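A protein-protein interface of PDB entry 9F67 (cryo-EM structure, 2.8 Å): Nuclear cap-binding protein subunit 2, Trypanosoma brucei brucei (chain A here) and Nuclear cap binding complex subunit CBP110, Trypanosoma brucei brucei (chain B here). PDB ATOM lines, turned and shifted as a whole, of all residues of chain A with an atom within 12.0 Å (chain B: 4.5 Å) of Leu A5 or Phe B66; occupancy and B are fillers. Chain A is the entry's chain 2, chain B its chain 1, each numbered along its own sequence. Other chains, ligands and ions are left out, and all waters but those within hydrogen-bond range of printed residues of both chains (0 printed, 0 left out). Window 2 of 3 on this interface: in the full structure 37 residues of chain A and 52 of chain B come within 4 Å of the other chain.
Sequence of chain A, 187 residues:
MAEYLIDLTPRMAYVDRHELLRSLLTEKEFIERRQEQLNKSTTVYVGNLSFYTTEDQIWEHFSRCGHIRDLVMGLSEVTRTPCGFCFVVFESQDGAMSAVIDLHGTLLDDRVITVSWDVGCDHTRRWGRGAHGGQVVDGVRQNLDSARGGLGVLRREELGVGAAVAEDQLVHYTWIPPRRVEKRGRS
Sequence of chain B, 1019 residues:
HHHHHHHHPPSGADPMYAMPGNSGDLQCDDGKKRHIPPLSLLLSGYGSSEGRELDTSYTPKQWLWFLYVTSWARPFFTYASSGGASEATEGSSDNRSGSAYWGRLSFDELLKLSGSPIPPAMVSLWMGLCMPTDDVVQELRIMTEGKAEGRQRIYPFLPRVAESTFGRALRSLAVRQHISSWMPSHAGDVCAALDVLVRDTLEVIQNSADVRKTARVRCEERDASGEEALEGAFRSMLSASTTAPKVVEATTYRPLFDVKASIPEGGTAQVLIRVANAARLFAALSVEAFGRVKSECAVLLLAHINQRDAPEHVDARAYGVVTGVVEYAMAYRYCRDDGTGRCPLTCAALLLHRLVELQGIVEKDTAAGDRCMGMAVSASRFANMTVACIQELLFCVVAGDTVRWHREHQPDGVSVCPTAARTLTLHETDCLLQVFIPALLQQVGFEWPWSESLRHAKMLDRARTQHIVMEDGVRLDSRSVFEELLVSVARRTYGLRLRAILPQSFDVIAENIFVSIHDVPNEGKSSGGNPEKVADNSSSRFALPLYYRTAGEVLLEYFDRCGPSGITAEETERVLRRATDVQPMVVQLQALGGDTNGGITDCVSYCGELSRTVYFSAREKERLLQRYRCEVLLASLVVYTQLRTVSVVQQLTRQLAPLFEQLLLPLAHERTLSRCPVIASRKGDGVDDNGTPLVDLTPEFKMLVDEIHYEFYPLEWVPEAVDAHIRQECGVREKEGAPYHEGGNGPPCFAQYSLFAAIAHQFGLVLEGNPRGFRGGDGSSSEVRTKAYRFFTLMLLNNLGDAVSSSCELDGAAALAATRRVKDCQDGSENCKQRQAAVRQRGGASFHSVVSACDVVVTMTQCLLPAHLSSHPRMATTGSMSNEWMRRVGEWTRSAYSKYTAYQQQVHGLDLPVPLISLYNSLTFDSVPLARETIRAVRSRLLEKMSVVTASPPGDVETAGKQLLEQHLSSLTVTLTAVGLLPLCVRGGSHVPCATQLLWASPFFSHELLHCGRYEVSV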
ATOM      1  N   MET A   1      -9.706  -7.794  19.787  1.00  0.00           N
ATOM      2  CA  MET A   1     -10.887  -6.906  19.898  1.00  0.00           C
ATOM      3  C   MET A   1     -12.043  -7.518  19.099  1.00  0.00           C
ATOM      4  O   MET A   1     -13.017  -7.960  19.729  1.00  0.00           O
ATOM      5  CB  MET A   1     -10.574  -5.561  19.263  1.00  0.00           C
ATOM      6  CG  MET A   1      -9.693  -4.648  20.068  1.00  0.00           C
ATOM      7  SD  MET A   1     -10.299  -4.163  21.676  1.00  0.00           S
ATOM      8  CE  MET A   1      -9.770  -2.455  21.666  1.00  0.00           C
ATOM      9  N   ALA A   2     -11.957  -7.509  17.761  1.00  0.00           N
ATOM     10  CA  ALA A   2     -13.017  -8.170  16.992  1.00  0.00           C
ATOM     11  C   ALA A   2     -12.902  -9.661  17.248  1.00  0.00           C
ATOM     12  O   ALA A   2     -13.844 -10.403  16.917  1.00  0.00           O
ATOM     13  CB  ALA A   2     -12.885  -7.835  15.546  1.00  0.00           C
ATOM     14  N   GLU A   3     -11.799 -10.082  17.851  1.00  0.00           N
ATOM     15  CA  GLU A   3     -11.614 -11.503  18.208  1.00  0.00           C
ATOM     16  C   GLU A   3     -12.297 -11.740  19.548  1.00  0.00           C
ATOM     17  O   GLU A   3     -12.033 -12.774  20.171  1.00  0.00           O
ATOM     18  CB  GLU A   3     -10.118 -11.772  18.254  1.00  0.00           C
ATOM     19  CG  GLU A   3      -9.311 -10.674  18.936  1.00  0.00           C
ATOM     20  CD  GLU A   3      -8.436  -9.906  17.963  1.00  0.00           C
ATOM     21  OE1 GLU A   3      -9.003  -9.191  17.109  1.00  0.00           O
ATOM     22  OE2 GLU A   3      -7.198 -10.014  18.065  1.00  0.00           O
ATOM     23  N   TYR A   4     -13.125 -10.801  19.969  1.00  0.00           N
ATOM     24  CA  TYR A   4     -13.853 -10.913  21.245  1.00  0.00           C
ATOM     25  C   TYR A   4     -15.291 -10.670  20.937  1.00  0.00           C
ATOM     26  O   TYR A   4     -16.125 -10.710  21.850  1.00  0.00           O
ATOM     27  CB  TYR A   4     -13.344  -9.827  22.181  1.00  0.00           C
ATOM     28  CG  TYR A   4     -11.975 -10.025  22.804  1.00  0.00           C
ATOM     29  CD1 TYR A   4     -11.790 -10.917  23.846  1.00  0.00           C
ATOM     30  CD2 TYR A   4     -10.889  -9.271  22.388  1.00  0.00           C
ATOM     31  CE1 TYR A   4     -10.554 -11.077  24.444  1.00  0.00           C
ATOM     32  CE2 TYR A   4      -9.650  -9.419  22.981  1.00  0.00           C
ATOM     33  CZ  TYR A   4      -9.481 -10.328  24.007  1.00  0.00           C
ATOM     34  OH  TYR A   4      -8.261 -10.490  24.595  1.00  0.00           O
ATOM     35  N   LEU A   5     -15.588 -10.419  19.668  1.00  0.00           N
ATOM     36  CA  LEU A   5     -16.977 -10.166  19.232  1.00  0.00           C
ATOM     37  C   LEU A   5     -17.349 -11.169  18.136  1.00  0.00           C
ATOM     38  O   LEU A   5     -18.546 -11.341  17.888  1.00  0.00           O
ATOM     39  CB  LEU A   5     -17.121  -8.728  18.749  1.00  0.00           C
ATOM     40  CG  LEU A   5     -16.927  -7.614  19.775  1.00  0.00           C
ATOM     41  CD1 LEU A   5     -16.979  -6.328  18.991  1.00  0.00           C
ATOM     42  CD2 LEU A   5     -18.016  -7.637  20.824  1.00  0.00           C
ATOM     43  N   ILE A   6     -16.372 -11.779  17.485  1.00  0.00           N
ATOM     44  CA  ILE A   6     -16.637 -12.845  16.485  1.00  0.00           C
ATOM     45  C   ILE A   6     -16.018 -14.124  17.049  1.00  0.00           C
ATOM     46  O   ILE A   6     -14.847 -14.063  17.438  1.00  0.00           O
ATOM     47  CB  ILE A   6     -16.030 -12.453  15.136  1.00  0.00           C
ATOM     48  CG1 ILE A   6     -16.332 -11.000  14.779  1.00  0.00           C
ATOM     49  CG2 ILE A   6     -16.488 -13.411  14.039  1.00  0.00           C
ATOM     50  CD1 ILE A   6     -17.761 -10.756  14.330  1.00  0.00           C
ATOM     51  N   ASP A   7     -16.667 -15.268  17.037  1.00  0.00           N
ATOM     52  CA  ASP A   7     -15.960 -16.453  17.587  1.00  0.00           C
ATOM     53  C   ASP A   7     -15.044 -17.008  16.536  1.00  0.00           C
ATOM     54  O   ASP A   7     -15.509 -17.736  15.668  1.00  0.00           O
ATOM     55  CB  ASP A   7     -16.816 -17.646  17.915  1.00  0.00           C
ATOM     56  CG  ASP A   7     -16.296 -18.492  19.062  1.00  0.00           C
ATOM     57  OD1 ASP A   7     -15.273 -18.098  19.656  1.00  0.00           O
ATOM     58  OD2 ASP A   7     -16.920 -19.530  19.356  1.00  0.00           O
ATOM     59  N   LEU A   8     -13.758 -16.649  16.597  1.00  0.00           N
ATOM     60  CA  LEU A   8     -12.791 -17.084  15.553  1.00  0.00           C
ATOM     61  C   LEU A   8     -12.135 -18.411  15.962  1.00  0.00           C
ATOM     62  O   LEU A   8     -11.049 -18.723  15.426  1.00  0.00           O
ATOM     63  CB  LEU A   8     -11.743 -15.994  15.347  1.00  0.00           C
ATOM     64  CG  LEU A   8     -12.279 -14.596  15.024  1.00  0.00           C
ATOM     65  CD1 LEU A   8     -11.143 -13.596  15.092  1.00  0.00           C
ATOM     66  CD2 LEU A   8     -12.914 -14.583  13.645  1.00  0.00           C
ATOM     67  N   THR A   9     -12.770 -19.159  16.866  1.00  0.00           N
ATOM     68  CA  THR A   9     -12.195 -20.437  17.340  1.00  0.00           C
ATOM     69  C   THR A   9     -11.916 -21.338  16.155  1.00  0.00           C
ATOM     70  O   THR A   9     -12.792 -21.450  15.271  1.00  0.00           O
ATOM     71  CB  THR A   9     -13.152 -21.092  18.335  1.00  0.00           C
ATOM     72  OG1 THR A   9     -14.459 -20.818  17.839  1.00  0.00           O
ATOM     73  CG2 THR A   9     -12.988 -20.547  19.742  1.00  0.00           C
ATOM     74  N   ARG A  11     -11.978 -24.162  13.581  1.00  0.00           N
ATOM     75  CA  ARG A  11     -13.101 -25.102  13.321  1.00  0.00           C
ATOM     76  C   ARG A  11     -12.844 -25.850  12.005  1.00  0.00           C
ATOM     77  O   ARG A  11     -12.145 -25.292  11.130  1.00  0.00           O
ATOM     78  CB  ARG A  11     -14.435 -24.350  13.259  1.00  0.00           C
ATOM     79  CG  ARG A  11     -14.893 -23.766  14.589  1.00  0.00           C
ATOM     80  CD  ARG A  11     -16.074 -22.820  14.440  1.00  0.00           C
ATOM     81  NE  ARG A  11     -16.416 -22.138  15.693  1.00  0.00           N
ATOM     82  CZ  ARG A  11     -16.828 -22.730  16.808  1.00  0.00           C
ATOM     83  NH1 ARG A  11     -17.203 -23.998  16.790  1.00  0.00           N
ATOM     84  NH2 ARG A  11     -16.877 -22.049  17.937  1.00  0.00           N
ATOM     85  N   MET A  97      -3.737 -18.278  13.058  1.00  0.00           N
ATOM     86  CA  MET A  97      -4.963 -17.446  13.141  1.00  0.00           C
ATOM     87  C   MET A  97      -4.826 -16.309  12.128  1.00  0.00           C
ATOM     88  O   MET A  97      -5.807 -16.015  11.416  1.00  0.00           O
ATOM     89  CB  MET A  97      -5.073 -16.836  14.539  1.00  0.00           C
ATOM     90  CG  MET A  97      -5.816 -17.685  15.546  1.00  0.00           C
ATOM     91  SD  MET A  97      -7.573 -17.883  15.171  1.00  0.00           S
ATOM     92  CE  MET A  97      -8.227 -18.077  16.827  1.00  0.00           C
ATOM     93  N   ILE A 101      -7.450 -15.749   8.521  1.00  0.00           N
ATOM     94  CA  ILE A 101      -8.261 -14.525   8.256  1.00  0.00           C
ATOM     95  C   ILE A 101      -7.680 -13.720   7.091  1.00  0.00           C
ATOM     96  O   ILE A 101      -8.449 -13.355   6.178  1.00  0.00           O
ATOM     97  CB  ILE A 101      -8.334 -13.664   9.533  1.00  0.00           C
ATOM     98  CG1 ILE A 101      -8.837 -14.466  10.736  1.00  0.00           C
ATOM     99  CG2 ILE A 101      -9.171 -12.416   9.297  1.00  0.00           C
ATOM    100  CD1 ILE A 101     -10.224 -15.034  10.558  1.00  0.00           C
ATOM    101  N   GLN B  62     -18.328  -8.612  31.065  1.00  0.00           N
ATOM    102  CA  GLN B  62     -18.471  -8.837  29.602  1.00  0.00           C
ATOM    103  C   GLN B  62     -18.982  -7.558  28.922  1.00  0.00           C
ATOM    104  O   GLN B  62     -18.469  -7.228  27.832  1.00  0.00           O
ATOM    105  CB  GLN B  62     -19.369 -10.058  29.391  1.00  0.00           C
ATOM    106  CG  GLN B  62     -18.747 -11.320  29.970  1.00  0.00           C
ATOM    107  CD  GLN B  62     -19.651 -12.528  29.975  1.00  0.00           C
ATOM    108  OE1 GLN B  62     -20.816 -12.463  29.595  1.00  0.00           O
ATOM    109  NE2 GLN B  62     -19.129 -13.640  30.463  1.00  0.00           N
ATOM    110  N   TRP B  63     -19.919  -6.847  29.559  1.00  0.00           N
ATOM    111  CA  TRP B  63     -20.416  -5.574  28.973  1.00  0.00           C
ATOM    112  C   TRP B  63     -19.282  -4.555  28.841  1.00  0.00           C
ATOM    113  O   TRP B  63     -19.190  -3.937  27.769  1.00  0.00           O
ATOM    114  CB  TRP B  63     -21.576  -4.986  29.787  1.00  0.00           C
ATOM    115  CG  TRP B  63     -22.886  -5.686  29.615  1.00  0.00           C
ATOM    116  CD1 TRP B  63     -23.631  -6.304  30.577  1.00  0.00           C
ATOM    117  CD2 TRP B  63     -23.642  -5.786  28.396  1.00  0.00           C
ATOM    118  NE1 TRP B  63     -24.786  -6.800  30.034  1.00  0.00           N
ATOM    119  CE2 TRP B  63     -24.821  -6.498  28.699  1.00  0.00           C
ATOM    120  CE3 TRP B  63     -23.436  -5.352  27.081  1.00  0.00           C
ATOM    121  CZ2 TRP B  63     -25.782  -6.788  27.733  1.00  0.00           C
ATOM    122  CZ3 TRP B  63     -24.388  -5.638  26.128  1.00  0.00           C
ATOM    123  CH2 TRP B  63     -25.545  -6.347  26.452  1.00  0.00           C
ATOM    124  N   LEU B  64     -18.418  -4.420  29.851  1.00  0.00           N
ATOM    125  CA  LEU B  64     -17.386  -3.356  29.736  1.00  0.00           C
ATOM    126  C   LEU B  64     -16.497  -3.660  28.529  1.00  0.00           C
ATOM    127  O   LEU B  64     -16.183  -2.718  27.780  1.00  0.00           O
ATOM    128  CB  LEU B  64     -16.544  -3.296  31.014  1.00  0.00           C
ATOM    129  CG  LEU B  64     -17.269  -2.823  32.270  1.00  0.00           C
ATOM    130  CD1 LEU B  64     -16.267  -2.483  33.361  1.00  0.00           C
ATOM    131  CD2 LEU B  64     -18.135  -1.612  31.957  1.00  0.00           C
ATOM    132  N   TRP B  65     -16.110  -4.926  28.359  1.00  0.00           N
ATOM    133  CA  TRP B  65     -15.180  -5.250  27.248  1.00  0.00           C
ATOM    134  C   TRP B  65     -15.869  -4.971  25.908  1.00  0.00           C
ATOM    135  O   TRP B  65     -15.215  -4.401  25.016  1.00  0.00           O
ATOM    136  CB  TRP B  65     -14.701  -6.699  27.333  1.00  0.00           C
ATOM    137  CG  TRP B  65     -13.585  -6.948  26.371  1.00  0.00           C
ATOM    138  CD1 TRP B  65     -13.576  -7.820  25.324  1.00  0.00           C
ATOM    139  CD2 TRP B  65     -12.289  -6.324  26.391  1.00  0.00           C
ATOM    140  NE1 TRP B  65     -12.372  -7.762  24.681  1.00  0.00           N
ATOM    141  CE2 TRP B  65     -11.558  -6.863  25.312  1.00  0.00           C
ATOM    142  CE3 TRP B  65     -11.676  -5.368  27.208  1.00  0.00           C
ATOM    143  CZ2 TRP B  65     -10.251  -6.476  25.030  1.00  0.00           C
ATOM    144  CZ3 TRP B  65     -10.384  -4.988  26.929  1.00  0.00           C
ATOM    145  CH2 TRP B  65      -9.683  -5.534  25.855  1.00  0.00           C
ATOM    146  N   PHE B  66     -17.144  -5.352  25.783  1.00  0.00           N
ATOM    147  CA  PHE B  66     -17.919  -5.078  24.545  1.00  0.00           C
ATOM    148  C   PHE B  66     -17.901  -3.576  24.277  1.00  0.00           C
ATOM    149  O   PHE B  66     -17.746  -3.164  23.110  1.00  0.00           O
ATOM    150  CB  PHE B  66     -19.354  -5.579  24.723  1.00  0.00           C
ATOM    151  CG  PHE B  66     -20.323  -5.192  23.635  1.00  0.00           C
ATOM    152  CD1 PHE B  66     -20.114  -5.565  22.318  1.00  0.00           C
ATOM    153  CD2 PHE B  66     -21.460  -4.459  23.933  1.00  0.00           C
ATOM    154  CE1 PHE B  66     -21.010  -5.209  21.324  1.00  0.00           C
ATOM    155  CE2 PHE B  66     -22.358  -4.104  22.940  1.00  0.00           C
ATOM    156  CZ  PHE B  66     -22.132  -4.478  21.637  1.00  0.00           C
ATOM    157  N   LEU B  67     -18.037  -2.787  25.339  1.00  0.00           N
ATOM    158  CA  LEU B  67     -18.091  -1.339  25.204  1.00  0.00           C
ATOM    159  C   LEU B  67     -16.675  -0.895  24.868  1.00  0.00           C
ATOM    160  O   LEU B  67     -16.544  -0.062  23.987  1.00  0.00           O
ATOM    161  CB  LEU B  67     -18.728  -0.715  26.443  1.00  0.00           C
ATOM    162  CG  LEU B  67     -20.152  -1.140  26.771  1.00  0.00           C
ATOM    163  CD1 LEU B  67     -20.752  -0.187  27.778  1.00  0.00           C
ATOM    164  CD2 LEU B  67     -21.004  -1.179  25.523  1.00  0.00           C
ATOM    165  N   TYR B  68     -15.654  -1.484  25.429  1.00  0.00           N
ATOM    166  CA  TYR B  68     -14.282  -1.060  25.194  1.00  0.00           C
ATOM    167  C   TYR B  68     -13.897  -1.240  23.736  1.00  0.00           C
ATOM    168  O   TYR B  68     -13.239  -0.374  23.148  1.00  0.00           O
ATOM    169  CB  TYR B  68     -13.324  -1.835  26.090  1.00  0.00           C
ATOM    170  CG  TYR B  68     -11.882  -1.474  25.861  1.00  0.00           C
ATOM    171  CD1 TYR B  68     -11.357  -0.303  26.373  1.00  0.00           C
ATOM    172  CD2 TYR B  68     -11.049  -2.289  25.121  1.00  0.00           C
ATOM    173  CE1 TYR B  68     -10.048   0.037  26.169  1.00  0.00           C
ATOM    174  CE2 TYR B  68      -9.737  -1.952  24.908  1.00  0.00           C
ATOM    175  CZ  TYR B  68      -9.243  -0.788  25.435  1.00  0.00           C
ATOM    176  OH  TYR B  68      -7.931  -0.451  25.224  1.00  0.00           O
ATOM    177  N   VAL B  69     -14.304  -2.355  23.131  1.00  0.00           N
ATOM    178  CA  VAL B  69     -13.980  -2.579  21.728  1.00  0.00           C
ATOM    179  C   VAL B  69     -14.870  -1.789  20.775  1.00  0.00           C
ATOM    180  O   VAL B  69     -14.372  -1.276  19.766  1.00  0.00           O
ATOM    181  CB  VAL B  69     -14.055  -4.071  21.372  1.00  0.00           C
ATOM    182  CG1 VAL B  69     -13.511  -4.306  19.977  1.00  0.00           C
ATOM    183  CG2 VAL B  69     -13.264  -4.880  22.361  1.00  0.00           C
ATOM    184  N   THR B  70     -16.172  -1.671  21.050  1.00  0.00           N
ATOM    185  CA  THR B  70     -17.123  -1.158  20.067  1.00  0.00           C
ATOM    186  C   THR B  70     -17.961  -0.003  20.622  1.00  0.00           C
ATOM    187  O   THR B  70     -19.180   0.026  20.501  1.00  0.00           O
ATOM    188  CB  THR B  70     -18.058  -2.260  19.577  1.00  0.00           C
ATOM    189  OG1 THR B  70     -19.074  -2.492  20.558  1.00  0.00           O
ATOM    190  CG2 THR B  70     -17.299  -3.545  19.345  1.00  0.00           C
ATOM    191  N   TRP B 126     -22.341  -8.612  16.588  1.00  0.00           N
ATOM    192  CA  TRP B 126     -22.056  -7.626  17.660  1.00  0.00           C
ATOM    193  C   TRP B 126     -22.802  -6.341  17.306  1.00  0.00           C
ATOM    194  O   TRP B 126     -23.025  -5.517  18.214  1.00  0.00           O
ATOM    195  CB  TRP B 126     -20.540  -7.441  17.827  1.00  0.00           C
ATOM    196  CG  TRP B 126     -19.813  -6.738  16.719  1.00  0.00           C
ATOM    197  CD1 TRP B 126     -18.871  -7.286  15.896  1.00  0.00           C
ATOM    198  CD2 TRP B 126     -19.785  -5.322  16.455  1.00  0.00           C
ATOM    199  NE1 TRP B 126     -18.354  -6.335  15.059  1.00  0.00           N
ATOM    200  CE2 TRP B 126     -18.887  -5.118  15.386  1.00  0.00           C
ATOM    201  CE3 TRP B 126     -20.457  -4.212  16.981  1.00  0.00           C
ATOM    202  CZ2 TRP B 126     -18.653  -3.857  14.840  1.00  0.00           C
ATOM    203  CZ3 TRP B 126     -20.231  -2.969  16.437  1.00  0.00           C
ATOM    204  CH2 TRP B 126     -19.339  -2.795  15.381  1.00  0.00           C
ATOM    205  N   LEU B 129     -26.420  -6.065  19.095  1.00  0.00           N
ATOM    206  CA  LEU B 129     -26.592  -6.284  20.557  1.00  0.00           C
ATOM    207  C   LEU B 129     -27.130  -5.021  21.242  1.00  0.00           C
ATOM    208  O   LEU B 129     -26.388  -4.022  21.310  1.00  0.00           O
ATOM    209  CB  LEU B 129     -25.252  -6.739  21.144  1.00  0.00           C
ATOM    210  CG  LEU B 129     -25.265  -7.079  22.632  1.00  0.00           C
ATOM    211  CD1 LEU B 129     -26.067  -8.347  22.879  1.00  0.00           C
ATOM    212  CD2 LEU B 129     -23.844  -7.278  23.131  1.00  0.00           C
ATOM    213  N   MET B 131     -28.163  -2.094  23.849  1.00  0.00           N
ATOM    214  CA  MET B 131     -27.386  -1.627  25.025  1.00  0.00           C
ATOM    215  C   MET B 131     -28.155  -2.015  26.293  1.00  0.00           C
ATOM    216  O   MET B 131     -29.400  -2.049  26.234  1.00  0.00           O
ATOM    217  CB  MET B 131     -27.129  -0.121  24.930  1.00  0.00           C
ATOM    218  CG  MET B 131     -26.077   0.148  23.876  1.00  0.00           C
ATOM    219  SD  MET B 131     -24.658  -0.953  24.122  1.00  0.00           S
ATOM    220  CE  MET B 131     -23.368  -0.045  23.275  1.00  0.00           C
ATOM    221  N   PHE B 290     -10.143  -3.585  15.348  1.00  0.00           N
ATOM    222  CA  PHE B 290     -10.664  -4.657  14.513  1.00  0.00           C
ATOM    223  C   PHE B 290      -9.659  -5.149  13.480  1.00  0.00           C
ATOM    224  O   PHE B 290     -10.051  -5.830  12.527  1.00  0.00           O
ATOM    225  CB  PHE B 290     -11.933  -4.199  13.791  1.00  0.00           C
ATOM    226  CG  PHE B 290     -13.114  -3.999  14.688  1.00  0.00           C
ATOM    227  CD1 PHE B 290     -13.149  -2.958  15.590  1.00  0.00           C
ATOM    228  CD2 PHE B 290     -14.197  -4.846  14.614  1.00  0.00           C
ATOM    229  CE1 PHE B 290     -14.236  -2.774  16.407  1.00  0.00           C
ATOM    230  CE2 PHE B 290     -15.285  -4.666  15.430  1.00  0.00           C
ATOM    231  CZ  PHE B 290     -15.304  -3.627  16.327  1.00  0.00           C
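Of the printed residues of chain B, Met A1 touches Tyr B68 and Val B69. Printed residues of chain B within 4 Å of Ile A6: Trp B126 (3.97 Å). Trp B63 touches none of the printed residues of chain A. No residue of chain A comes within 4 Å of Leu B67. Printed residues of chain A within 4 Å of Thr B70: Leu A5. Of the printed residues of chain A, Phe B290 touches Ala A2. The nearest printed residue of chain B that does not touch Leu A5 is Val B69 (4.1 Å). The nearest printed residue of chain B that does not touch Tyr A4 is Val B69 (5.0 Å).
Tyr B68 touches Met A1. Val B69 touches Met A1. Ala A2 touches Phe B290 (CB to CD2, 3.4 Å). Trp B65 touches Tyr A4. Leu A5 touches Phe B66 (CD2 to CD1, 3.3 Å). Leu A5 touches Thr B70 (CD1 to CG2, 2.8 Å). Leu A5 touches Trp B126 (CB to CD1, 3.6 Å). CD1 of Ile A6 touches CD1 of Trp B126, at 3.97 Å.
OE1 of Glu A3 sits close to N of Met A1 (3.1 Å). OG1 of Thr B70 is in hydrogen-bond range of O of Phe B66 (3.0 Å).
Hydrophobic or aromatic side chains of chain A within 4 Å of the printed part of chain B: Met A1, Ala A2, Tyr A4, Leu A5 and Ile A6. Of the 13 printed residues of chain B, 7 touch a printed residue of chain A. Printed residues of chain B that touch a printed residue of chain A: Trp B65, Phe B66, Tyr B68, Val B69, Thr B70, Trp B126 and Phe B290. Among the printed residues, 8 pairs touch across the chains.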
